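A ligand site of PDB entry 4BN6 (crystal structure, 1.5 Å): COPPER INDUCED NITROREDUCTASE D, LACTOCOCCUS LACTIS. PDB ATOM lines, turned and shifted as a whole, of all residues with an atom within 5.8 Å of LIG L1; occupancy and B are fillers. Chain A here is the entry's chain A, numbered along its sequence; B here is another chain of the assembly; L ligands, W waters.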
ATOM      1  N   ARG A   9      14.993  -6.808 -22.067  1.00  0.00           N
ATOM      2  CA  ARG A   9      14.711  -7.229 -23.441  1.00  0.00           C
ATOM      3  C   ARG A   9      13.875  -8.491 -23.412  1.00  0.00           C
ATOM      4  O   ARG A   9      14.257  -9.486 -22.794  1.00  0.00           O
ATOM      5  CB  ARG A   9      15.999  -7.501 -24.225  1.00  0.00           C
ATOM      6  CG  ARG A   9      15.769  -7.883 -25.694  1.00  0.00           C
ATOM      7  CD  ARG A   9      16.681  -9.006 -26.161  1.00  0.00           C
ATOM      8  NE  ARG A   9      16.633 -10.116 -25.225  1.00  0.00           N
ATOM      9  CZ  ARG A   9      15.696 -11.056 -25.192  1.00  0.00           C
ATOM     10  NH1 ARG A   9      14.715 -11.073 -26.096  1.00  0.00           N
ATOM     11  NH2 ARG A   9      15.732 -11.988 -24.260  1.00  0.00           N
ATOM     12  N   ARG A  10      12.729  -8.457 -24.097  1.00  0.00           N
ATOM     13  CA  ARG A  10      11.843  -9.611 -24.180  1.00  0.00           C
ATOM     14  C   ARG A  10      11.191  -9.673 -25.555  1.00  0.00           C
ATOM     15  O   ARG A  10      11.152  -8.688 -26.291  1.00  0.00           O
ATOM     16  CB  ARG A  10      10.765  -9.540 -23.098  1.00  0.00           C
ATOM     17  CG  ARG A  10      11.289  -9.624 -21.670  1.00  0.00           C
ATOM     18  CD  ARG A  10      11.896 -11.000 -21.317  1.00  0.00           C
ATOM     19  NE  ARG A  10      10.955 -12.085 -21.559  1.00  0.00           N
ATOM     20  CZ  ARG A  10       9.977 -12.437 -20.744  1.00  0.00           C
ATOM     21  NH1 ARG A  10       9.806 -11.805 -19.581  1.00  0.00           N
ATOM     22  NH2 ARG A  10       9.161 -13.428 -21.071  1.00  0.00           N
ATOM     23  N   THR A  11      10.677 -10.847 -25.876  1.00  0.00           N
ATOM     24  CA  THR A  11       9.847 -11.035 -27.063  1.00  0.00           C
ATOM     25  C   THR A  11       8.467 -10.447 -26.792  1.00  0.00           C
ATOM     26  O   THR A  11       7.738 -10.892 -25.898  1.00  0.00           O
ATOM     27  CB  THR A  11       9.717 -12.536 -27.400  1.00  0.00           C
ATOM     28  OG1 THR A  11      10.974 -13.019 -27.895  1.00  0.00           O
ATOM     29  CG2 THR A  11       8.637 -12.784 -28.453  1.00  0.00           C
ATOM     30  N   ILE A  12       8.127  -9.425 -27.568  1.00  0.00           N
ATOM     31  CA  ILE A  12       6.850  -8.746 -27.488  1.00  0.00           C
ATOM     32  C   ILE A  12       6.141  -8.894 -28.821  1.00  0.00           C
ATOM     33  O   ILE A  12       6.581  -8.365 -29.836  1.00  0.00           O
ATOM     34  CB  ILE A  12       7.018  -7.241 -27.195  1.00  0.00           C
ATOM     35  CG1 ILE A  12       7.824  -7.009 -25.910  1.00  0.00           C
ATOM     36  CG2 ILE A  12       5.668  -6.552 -27.107  1.00  0.00           C
ATOM     37  CD1 ILE A  12       7.193  -7.576 -24.656  1.00  0.00           C
ATOM     38  N   TYR A  13       5.032  -9.641 -28.818  1.00  0.00           N
ATOM     39  CA  TYR A  13       4.279  -9.869 -30.039  1.00  0.00           C
ATOM     40  C   TYR A  13       3.235  -8.793 -30.304  1.00  0.00           C
ATOM     41  O   TYR A  13       2.884  -8.538 -31.447  1.00  0.00           O
ATOM     42  CB  TYR A  13       3.603 -11.249 -30.006  1.00  0.00           C
ATOM     43  CG  TYR A  13       4.586 -12.384 -30.119  1.00  0.00           C
ATOM     44  CD1 TYR A  13       5.371 -12.539 -31.256  1.00  0.00           C
ATOM     45  CD2 TYR A  13       4.745 -13.314 -29.098  1.00  0.00           C
ATOM     46  CE1 TYR A  13       6.275 -13.551 -31.368  1.00  0.00           C
ATOM     47  CE2 TYR A  13       5.643 -14.355 -29.208  1.00  0.00           C
ATOM     48  CZ  TYR A  13       6.422 -14.468 -30.347  1.00  0.00           C
ATOM     49  OH  TYR A  13       7.327 -15.494 -30.472  1.00  0.00           O
ATOM     50  N   PHE A  91       2.350  -8.740 -37.115  1.00  0.00           N
ATOM     51  CA  PHE A  91       3.660  -8.242 -37.533  1.00  0.00           C
ATOM     52  C   PHE A  91       3.499  -6.935 -38.314  1.00  0.00           C
ATOM     53  O   PHE A  91       4.247  -5.981 -38.090  1.00  0.00           O
ATOM     54  CB  PHE A  91       4.380  -9.302 -38.383  1.00  0.00           C
ATOM     55  CG  PHE A  91       4.667 -10.578 -37.648  1.00  0.00           C
ATOM     56  CD1 PHE A  91       5.103 -10.566 -36.324  1.00  0.00           C
ATOM     57  CD2 PHE A  91       4.477 -11.803 -38.269  1.00  0.00           C
ATOM     58  CE1 PHE A  91       5.354 -11.752 -35.650  1.00  0.00           C
ATOM     59  CE2 PHE A  91       4.720 -12.997 -37.588  1.00  0.00           C
ATOM     60  CZ  PHE A  91       5.152 -12.965 -36.286  1.00  0.00           C
ATOM     61  N   VAL A 134      20.595  -9.290 -31.370  1.00  0.00           N
ATOM     62  CA  VAL A 134      20.210  -9.129 -29.970  1.00  0.00           C
ATOM     63  C   VAL A 134      20.684  -7.791 -29.403  1.00  0.00           C
ATOM     64  O   VAL A 134      20.020  -7.224 -28.540  1.00  0.00           O
ATOM     65  CB  VAL A 134      20.685 -10.288 -29.054  1.00  0.00           C
ATOM     66  CG1 VAL A 134      20.120 -11.614 -29.543  1.00  0.00           C
ATOM     67  CG2 VAL A 134      22.213 -10.328 -28.920  1.00  0.00           C
ATOM     68  N   TRP A 137      18.022  -5.499 -30.591  1.00  0.00           N
ATOM     69  CA  TRP A 137      16.817  -5.832 -29.831  1.00  0.00           C
ATOM     70  C   TRP A 137      16.869  -5.223 -28.414  1.00  0.00           C
ATOM     71  O   TRP A 137      15.897  -4.625 -27.945  1.00  0.00           O
ATOM     72  CB  TRP A 137      16.731  -7.355 -29.777  1.00  0.00           C
ATOM     73  CG  TRP A 137      15.423  -8.005 -29.400  1.00  0.00           C
ATOM     74  CD1 TRP A 137      14.315  -7.432 -28.863  1.00  0.00           C
ATOM     75  CD2 TRP A 137      15.149  -9.389 -29.543  1.00  0.00           C
ATOM     76  NE1 TRP A 137      13.336  -8.398 -28.658  1.00  0.00           N
ATOM     77  CE2 TRP A 137      13.837  -9.604 -29.078  1.00  0.00           C
ATOM     78  CE3 TRP A 137      15.881 -10.469 -30.024  1.00  0.00           C
ATOM     79  CZ2 TRP A 137      13.254 -10.871 -29.081  1.00  0.00           C
ATOM     80  CZ3 TRP A 137      15.306 -11.720 -30.028  1.00  0.00           C
ATOM     81  CH2 TRP A 137      14.000 -11.906 -29.565  1.00  0.00           C
ATOM     82  N   ASN A 148      10.129  -8.566 -31.715  1.00  0.00           N
ATOM     83  CA  ASN A 148      10.190 -10.017 -31.809  1.00  0.00           C
ATOM     84  C   ASN A 148      10.944 -10.384 -33.075  1.00  0.00           C
ATOM     85  O   ASN A 148      10.974  -9.616 -34.041  1.00  0.00           O
ATOM     86  CB  ASN A 148       8.790 -10.642 -31.759  1.00  0.00           C
ATOM     87  CG  ASN A 148       7.916 -10.219 -32.924  1.00  0.00           C
ATOM     88  OD1 ASN A 148       8.041 -10.741 -34.036  1.00  0.00           O
ATOM     89  ND2 ASN A 148       7.007  -9.280 -32.687  1.00  0.00           N
ATOM     90  N   LEU A 149      11.601 -11.549 -33.054  1.00  0.00           N
ATOM     91  CA  LEU A 149      12.497 -11.947 -34.115  1.00  0.00           C
ATOM     92  C   LEU A 149      11.893 -13.077 -34.947  1.00  0.00           C
ATOM     93  O   LEU A 149      11.597 -14.155 -34.427  1.00  0.00           O
ATOM     94  CB  LEU A 149      13.845 -12.386 -33.537  1.00  0.00           C
ATOM     95  CG  LEU A 149      14.919 -12.811 -34.542  1.00  0.00           C
ATOM     96  CD1 LEU A 149      15.373 -11.631 -35.375  1.00  0.00           C
ATOM     97  CD2 LEU A 149      16.088 -13.449 -33.830  1.00  0.00           C
ATOM     98  N   GLN A 150      11.720 -12.816 -36.234  1.00  0.00           N
ATOM     99  CA  GLN A 150      11.109 -13.786 -37.139  1.00  0.00           C
ATOM    100  C   GLN A 150      12.083 -14.293 -38.188  1.00  0.00           C
ATOM    101  O   GLN A 150      13.149 -13.695 -38.409  1.00  0.00           O
ATOM    102  CB  GLN A 150       9.902 -13.160 -37.829  1.00  0.00           C
ATOM    103  CG  GLN A 150       8.806 -12.735 -36.888  1.00  0.00           C
ATOM    104  CD  GLN A 150       8.414 -13.840 -35.932  1.00  0.00           C
ATOM    105  OE1 GLN A 150       8.279 -14.994 -36.324  1.00  0.00           O
ATOM    106  NE2 GLN A 150       8.260 -13.493 -34.661  1.00  0.00           N
ATOM    107  N   HIS A 151      11.700 -15.385 -38.835  1.00  0.00           N
ATOM    108  CA  HIS A 151      12.528 -16.056 -39.829  1.00  0.00           C
ATOM    109  C   HIS A 151      11.715 -16.549 -41.007  1.00  0.00           C
ATOM    110  O   HIS A 151      11.371 -17.733 -41.096  1.00  0.00           O
ATOM    111  CB  HIS A 151      13.290 -17.205 -39.166  1.00  0.00           C
ATOM    112  CG  HIS A 151      14.293 -16.728 -38.182  1.00  0.00           C
ATOM    113  ND1 HIS A 151      14.014 -16.612 -36.838  1.00  0.00           N
ATOM    114  CD2 HIS A 151      15.551 -16.255 -38.356  1.00  0.00           C
ATOM    115  CE1 HIS A 151      15.074 -16.104 -36.225  1.00  0.00           C
ATOM    116  NE2 HIS A 151      16.010 -15.886 -37.124  1.00  0.00           N
ATOM    117  N   ALA A 185       5.175  -9.108 -22.135  1.00  0.00           N
ATOM    118  CA  ALA A 185       5.759 -10.382 -22.468  1.00  0.00           C
ATOM    119  C   ALA A 185       5.082 -11.506 -21.684  1.00  0.00           C
ATOM    120  O   ALA A 185       4.528 -11.289 -20.611  1.00  0.00           O
ATOM    121  CB  ALA A 185       7.243 -10.369 -22.159  1.00  0.00           C
ATOM    122  N   LYS A 188       8.255 -16.887 -18.818  1.00  0.00           N
ATOM    123  CA  LYS A 188       9.441 -17.569 -19.343  1.00  0.00           C
ATOM    124  C   LYS A 188      10.184 -18.264 -18.209  1.00  0.00           C
ATOM    125  O   LYS A 188      10.432 -17.674 -17.163  1.00  0.00           O
ATOM    126  CB  LYS A 188      10.374 -16.587 -20.051  1.00  0.00           C
ATOM    127  CG  LYS A 188      11.619 -17.262 -20.606  1.00  0.00           C
ATOM    128  CD  LYS A 188      12.513 -16.289 -21.356  1.00  0.00           C
ATOM    129  CE  LYS A 188      13.052 -15.188 -20.471  1.00  0.00           C
ATOM    130  NZ  LYS A 188      14.133 -14.433 -21.162  1.00  0.00           N
ATOM    131  N   PHE B  35      19.903 -14.305 -19.092  1.00  0.00           N
ATOM    132  CA  PHE B  35      18.990 -13.343 -19.707  1.00  0.00           C
ATOM    133  C   PHE B  35      19.201 -13.177 -21.207  1.00  0.00           C
ATOM    134  O   PHE B  35      18.677 -12.245 -21.805  1.00  0.00           O
ATOM    135  CB  PHE B  35      19.085 -12.011 -18.963  1.00  0.00           C
ATOM    136  CG  PHE B  35      18.669 -12.104 -17.514  1.00  0.00           C
ATOM    137  CD1 PHE B  35      17.453 -12.690 -17.163  1.00  0.00           C
ATOM    138  CD2 PHE B  35      19.496 -11.661 -16.504  1.00  0.00           C
ATOM    139  CE1 PHE B  35      17.067 -12.801 -15.855  1.00  0.00           C
ATOM    140  CE2 PHE B  35      19.121 -11.768 -15.167  1.00  0.00           C
ATOM    141  CZ  PHE B  35      17.902 -12.342 -14.846  1.00  0.00           C
ATOM    142  N   SER B  36      19.928 -14.115 -21.831  1.00  0.00           N
ATOM    143  CA  SER B  36      20.117 -14.129 -23.271  1.00  0.00           C
ATOM    144  C   SER B  36      19.034 -14.953 -23.957  1.00  0.00           C
ATOM    145  O   SER B  36      18.677 -16.036 -23.486  1.00  0.00           O
ATOM    146  CB  SER B  36      21.485 -14.717 -23.634  1.00  0.00           C
ATOM    147  OG  SER B  36      22.541 -13.882 -23.188  1.00  0.00           O
ATOM    148  N   PRO B  37      18.491 -14.432 -25.063  1.00  0.00           N
ATOM    149  CA  PRO B  37      17.477 -15.190 -25.796  1.00  0.00           C
ATOM    150  C   PRO B  37      18.056 -16.322 -26.647  1.00  0.00           C
ATOM    151  O   PRO B  37      19.170 -16.213 -27.174  1.00  0.00           O
ATOM    152  CB  PRO B  37      16.835 -14.128 -26.676  1.00  0.00           C
ATOM    153  CG  PRO B  37      17.959 -13.202 -26.981  1.00  0.00           C
ATOM    154  CD  PRO B  37      18.792 -13.153 -25.729  1.00  0.00           C
ATOM    155  N   THR B  38      17.277 -17.391 -26.793  1.00  0.00           N
ATOM    156  CA  THR B  38      17.583 -18.523 -27.654  1.00  0.00           C
ATOM    157  C   THR B  38      16.293 -18.990 -28.315  1.00  0.00           C
ATOM    158  O   THR B  38      15.202 -18.850 -27.746  1.00  0.00           O
ATOM    159  CB  THR B  38      18.181 -19.705 -26.873  1.00  0.00           C
ATOM    160  OG1 THR B  38      17.328 -20.036 -25.778  1.00  0.00           O
ATOM    161  CG2 THR B  38      19.578 -19.367 -26.383  1.00  0.00           C
ATOM    162  N   ALA B  39      16.400 -19.542 -29.517  1.00  0.00           N
ATOM    163  CA  ALA B  39      15.224 -20.037 -30.221  1.00  0.00           C
ATOM    164  C   ALA B  39      14.425 -21.009 -29.338  1.00  0.00           C
ATOM    165  O   ALA B  39      14.995 -21.912 -28.736  1.00  0.00           O
ATOM    166  CB  ALA B  39      15.643 -20.723 -31.513  1.00  0.00           C
ATOM    167  N   PHE B  40      13.108 -20.797 -29.287  1.00  0.00           N
ATOM    168  CA  PHE B  40      12.208 -21.661 -28.508  1.00  0.00           C
ATOM    169  C   PHE B  40      12.566 -21.710 -27.023  1.00  0.00           C
ATOM    170  O   PHE B  40      12.172 -22.643 -26.319  1.00  0.00           O
ATOM    171  CB  PHE B  40      12.204 -23.091 -29.071  1.00  0.00           C
ATOM    172  CG  PHE B  40      11.408 -23.249 -30.331  1.00  0.00           C
ATOM    173  CD1 PHE B  40      11.974 -22.985 -31.573  1.00  0.00           C
ATOM    174  CD2 PHE B  40      10.085 -23.653 -30.273  1.00  0.00           C
ATOM    175  CE1 PHE B  40      11.220 -23.138 -32.729  1.00  0.00           C
ATOM    176  CE2 PHE B  40       9.341 -23.804 -31.428  1.00  0.00           C
ATOM    177  CZ  PHE B  40       9.907 -23.540 -32.657  1.00  0.00           C
ATOM    178  N   ASN B  41      13.303 -20.709 -26.554  1.00  0.00           N
ATOM    179  CA  ASN B  41      13.825 -20.724 -25.187  1.00  0.00           C
ATOM    180  C   ASN B  41      14.569 -22.018 -24.905  1.00  0.00           C
ATOM    181  O   ASN B  41      14.517 -22.553 -23.797  1.00  0.00           O
ATOM    182  CB  ASN B  41      12.687 -20.537 -24.167  1.00  0.00           C
ATOM    183  CG  ASN B  41      13.198 -20.153 -22.795  1.00  0.00           C
ATOM    184  OD1 ASN B  41      14.195 -19.445 -22.667  1.00  0.00           O
ATOM    185  ND2 ASN B  41      12.514 -20.604 -21.752  1.00  0.00           N
ATOM    186  N   TRP B 124      20.380 -21.548 -35.479  1.00  0.00           N
ATOM    187  CA  TRP B 124      19.966 -20.719 -34.344  1.00  0.00           C
ATOM    188  C   TRP B 124      20.829 -20.996 -33.116  1.00  0.00           C
ATOM    189  O   TRP B 124      21.055 -20.106 -32.299  1.00  0.00           O
ATOM    190  CB  TRP B 124      18.491 -20.946 -34.024  1.00  0.00           C
ATOM    191  CG  TRP B 124      17.566 -20.440 -35.094  1.00  0.00           C
ATOM    192  CD1 TRP B 124      17.803 -19.434 -35.978  1.00  0.00           C
ATOM    193  CD2 TRP B 124      16.260 -20.941 -35.392  1.00  0.00           C
ATOM    194  NE1 TRP B 124      16.714 -19.263 -36.806  1.00  0.00           N
ATOM    195  CE2 TRP B 124      15.751 -20.183 -36.469  1.00  0.00           C
ATOM    196  CE3 TRP B 124      15.459 -21.960 -34.846  1.00  0.00           C
ATOM    197  CZ2 TRP B 124      14.488 -20.410 -37.003  1.00  0.00           C
ATOM    198  CZ3 TRP B 124      14.214 -22.170 -35.381  1.00  0.00           C
ATOM    199  CH2 TRP B 124      13.744 -21.400 -36.453  1.00  0.00           C
ATOM    200  N   GLN B 127      24.008 -19.004 -33.684  1.00  0.00           N
ATOM    201  CA  GLN B 127      23.691 -17.623 -33.355  1.00  0.00           C
ATOM    202  C   GLN B 127      23.634 -17.470 -31.840  1.00  0.00           C
ATOM    203  O   GLN B 127      24.186 -16.507 -31.280  1.00  0.00           O
ATOM    204  CB  GLN B 127      22.374 -17.200 -34.031  1.00  0.00           C
ATOM    205  CG  GLN B 127      22.495 -17.178 -35.550  1.00  0.00           C
ATOM    206  CD  GLN B 127      21.190 -16.906 -36.268  1.00  0.00           C
ATOM    207  OE1 GLN B 127      20.127 -16.809 -35.648  1.00  0.00           O
ATOM    208  NE2 GLN B 127      21.260 -16.781 -37.580  1.00  0.00           N
ATOM    209  N   GLY B 128      23.020 -18.432 -31.166  1.00  0.00           N
ATOM    210  CA  GLY B 128      22.933 -18.423 -29.720  1.00  0.00           C
ATOM    211  C   GLY B 128      24.281 -18.389 -29.020  1.00  0.00           C
ATOM    212  O   GLY B 128      24.449 -17.746 -27.983  1.00  0.00           O
ATOM    213  N   ILE B 131      25.562 -14.877 -29.271  1.00  0.00           N
ATOM    214  CA  ILE B 131      24.762 -14.077 -28.355  1.00  0.00           C
ATOM    215  C   ILE B 131      25.269 -14.184 -26.919  1.00  0.00           C
ATOM    216  O   ILE B 131      25.542 -13.159 -26.273  1.00  0.00           O
ATOM    217  CB  ILE B 131      23.276 -14.493 -28.442  1.00  0.00           C
ATOM    218  CG1 ILE B 131      22.682 -14.007 -29.771  1.00  0.00           C
ATOM    219  CG2 ILE B 131      22.469 -13.939 -27.271  1.00  0.00           C
ATOM    220  CD1 ILE B 131      21.405 -14.716 -30.164  1.00  0.00           C
HETATM  221  N1  LIG L   1      10.618 -16.064 -31.936  1.00  0.00           N
HETATM  222  C1  LIG L   1       9.565 -16.101 -33.008  1.00  0.00           C
HETATM  223  O1  LIG L   1       8.453 -15.747 -32.784  1.00  0.00           O
HETATM  224  N2  LIG L   1       9.914 -16.598 -34.310  1.00  0.00           N
HETATM  225  C2  LIG L   1      11.180 -17.039 -34.595  1.00  0.00           C
HETATM  226  O2  LIG L   1      11.472 -17.335 -35.709  1.00  0.00           O
HETATM  227  C3  LIG L   1      12.202 -17.001 -33.543  1.00  0.00           C
HETATM  228  N3  LIG L   1      13.387 -17.430 -33.764  1.00  0.00           N
HETATM  229  C4  LIG L   1      14.469 -17.078 -32.795  1.00  0.00           C
HETATM  230  C5  LIG L   1      15.906 -17.271 -33.225  1.00  0.00           C
HETATM  231  C6  LIG L   1      16.876 -16.931 -32.395  1.00  0.00           C
HETATM  232  C7  LIG L   1      18.336 -17.140 -32.803  1.00  0.00           C
HETATM  233  C8  LIG L   1      16.554 -16.339 -31.029  1.00  0.00           C
HETATM  234  C9  LIG L   1      17.717 -15.866 -30.153  1.00  0.00           C
HETATM  235  C10 LIG L   1      15.303 -16.170 -30.650  1.00  0.00           C
HETATM  236  C11 LIG L   1      14.166 -16.564 -31.580  1.00  0.00           C
HETATM  237  N4  LIG L   1      12.796 -16.413 -31.185  1.00  0.00           N
HETATM  238  C12 LIG L   1      11.841 -16.481 -32.193  1.00  0.00           C
HETATM  239  C13 LIG L   1      12.430 -15.868 -29.893  1.00  0.00           C
HETATM  240  C14 LIG L   1      12.735 -16.877 -28.777  1.00  0.00           C
HETATM  241  O3  LIG L   1      11.781 -17.901 -28.774  1.00  0.00           O
HETATM  242  C15 LIG L   1      12.739 -16.102 -27.462  1.00  0.00           C
HETATM  243  O4  LIG L   1      13.850 -15.251 -27.535  1.00  0.00           O
HETATM  244  C16 LIG L   1      12.853 -17.043 -26.255  1.00  0.00           C
HETATM  245  O5  LIG L   1      11.666 -17.777 -26.067  1.00  0.00           O
HETATM  246  C17 LIG L   1      13.134 -16.233 -24.981  1.00  0.00           C
HETATM  247  O6  LIG L   1      12.096 -15.315 -24.756  1.00  0.00           O
HETATM  248  P1  LIG L   1      12.406 -13.706 -24.648  1.00  0.00           P
HETATM  249  O7  LIG L   1      13.459 -13.486 -23.657  1.00  0.00           O
HETATM  250  O8  LIG L   1      12.909 -13.198 -26.109  1.00  0.00           O
HETATM  251  O9  LIG L   1      11.021 -12.994 -24.185  1.00  0.00           O
HETATM  252  C1  LG2 L   2       9.439 -24.293 -36.686  1.00  0.00           C
HETATM  253 CL1  LG2 L   2       9.165 -25.629 -35.684  1.00  0.00          CL
HETATM  254 CL2  LG2 L   2      11.015 -23.754 -36.707  1.00  0.00          CL
HETATM  255  C2  LG2 L   2       8.432 -23.197 -36.563  1.00  0.00           C
HETATM  256  O1  LG2 L   2       7.560 -23.251 -35.718  1.00  0.00           O
HETATM  257  N1  LG2 L   2       8.526 -22.113 -37.449  1.00  0.00           N
HETATM  258  C3  LG2 L   2       7.576 -21.003 -37.377  1.00  0.00           C
HETATM  259  C4  LG2 L   2       6.787 -20.817 -38.658  1.00  0.00           C
HETATM  260  O2  LG2 L   2       6.541 -19.559 -39.052  1.00  0.00           O
HETATM  261  C5  LG2 L   2       8.272 -19.694 -37.046  1.00  0.00           C
HETATM  262  O3  LG2 L   2       9.193 -19.388 -38.013  1.00  0.00           O
HETATM  263  C6  LG2 L   2       8.991 -19.733 -35.638  1.00  0.00           C
HETATM  264  C7  LG2 L   2       8.278 -19.523 -34.477  1.00  0.00           C
HETATM  265  C8  LG2 L   2       8.931 -19.551 -33.211  1.00  0.00           C
HETATM  266  C9  LG2 L   2      10.338 -19.801 -33.148  1.00  0.00           C
HETATM  267  N2  LG2 L   2      11.072 -19.821 -31.819  1.00  0.00           N
HETATM  268  O4  LG2 L   2      12.375 -19.804 -31.826  1.00  0.00           O
HETATM  269  O5  LG2 L   2      10.465 -19.851 -30.767  1.00  0.00           O
HETATM  270  C10 LG2 L   2      11.050 -20.004 -34.302  1.00  0.00           C
HETATM  271  C11 LG2 L   2      10.385 -19.970 -35.575  1.00  0.00           C
HETATM  272  O   HOH W   1       9.206 -14.642 -23.587  1.00  0.00           O
HETATM  273  O   HOH W   2      10.873 -13.225 -30.842  1.00  0.00           O
HETATM  274  O   HOH W   3       9.309 -16.832 -38.140  1.00  0.00           O
HETATM  275  O   HOH W   4       9.512 -17.282 -24.489  1.00  0.00           O
HETATM  276  O   HOH W   5       9.152 -16.880 -28.806  1.00  0.00           O
HETATM  277  O   HOH W   6       5.875 -16.620 -34.040  1.00  0.00           O
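NE2 of His 151 sits at hydrogen-bond distance from NE1 of Trp 124 of chain B (3.5 Å). The side-chain amide nitrogen (NE2) of Gln 150 is in hydrogen-bond range of the side-chain amide oxygen (OD1) of Asn 148 (2.8 Å). The indole nitrogen (NE1) of Trp 137 is in hydrogen-bond range of the backbone carbonyl oxygen (O) of Arg 10 (3.2 Å).
CZ2 of Trp 137 touches O8 of LIG L1, at 3.8 Å. Pro 37 of chain B touches LIG L1. O of Thr 38 of chain B touches C16 of LIG L1, 3.3 Å away. Ala 39 of chain B touches LIG L1 (N to C8, 3.5 Å). CD1 of Trp 124 of chain B touches C7 of LIG L1, at 3.95 Å. Gln 127 of chain B touches LIG L1 (OE1 to C7, 3.4 Å). Ile 131 of chain B touches LIG L1. Of the 25 residues printed, 17 come within 4 Å of LIG L1. The nearest printed residue that does not touch LIG L1 is Val 134 (4.9 Å).
O3 of LIG L1 sits at hydrogen-bond distance from O5 of LG2 L2, at 3.1 Å.
Water W1 bridges O9 of LIG L1 (2.5 Å) and NH2 of Arg 10 (2.8 Å). Water W5 lies within hydrogen-bond range of an oxygen (O3) of LIG L1 and the side-chain hydroxyl of Tyr 13. Water W2 lies within hydrogen-bond range of the backbone NH (N) of Leu 149 (2.9 Å), the side-chain hydroxyl (OG1) of Thr 11 (3.0 Å) and a nitrogen (N1) of LIG L1 (3.1 Å). Water W3 lies within hydrogen-bond range of an oxygen (O3) of LG2 L2 (2.6 Å), the side-chain amide oxygen (OE1) of Gln 150 (2.8 Å), the backbone NH (N) of His 151 (2.9 Å) and an oxygen (O2) of LIG L1 (3.3 Å).
An oxygen (O4) of LG2 L2 is in hydrogen-bond range of the backbone NH (N) of Phe 40 of chain B, at 2.8 Å. O2 of LIG L1 is in hydrogen-bond range of ND1 of His 151 (2.9 Å). An oxygen (O1) of LIG L1 is in hydrogen-bond range of the side-chain hydroxyl of Tyr 13 (2.6 Å). The backbone carbonyl oxygen of Leu 149 sits close to a nitrogen (N2) of LIG L1 (3.0 Å). An oxygen (O7) of LIG L1 lies within salt-bridge range of the side-chain amino group of Lys 188, 2.8 Å away. NH2 of Arg 9 is in salt-bridge range of O7 of LIG L1, at 2.8 Å. O9 of LIG L1 is in salt-bridge range of NE of Arg 10, 2.8 Å away. O1 of LIG L1 sits at hydrogen-bond distance from NE2 of Gln 150. The side-chain hydroxyl of Thr 11 sits at hydrogen-bond distance from an oxygen (O8) of LIG L1 (2.6 Å). N of Phe 40 of chain B is in hydrogen-bond range of O3 of LIG L1, at 3.2 Å. The backbone NH of Asn 41 of chain B lies within hydrogen-bond range of an oxygen (O5) of LIG L1, 3.4 Å away. O9 of LIG L1 lies within hydrogen-bond range of N of Thr 11 (2.8 Å).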
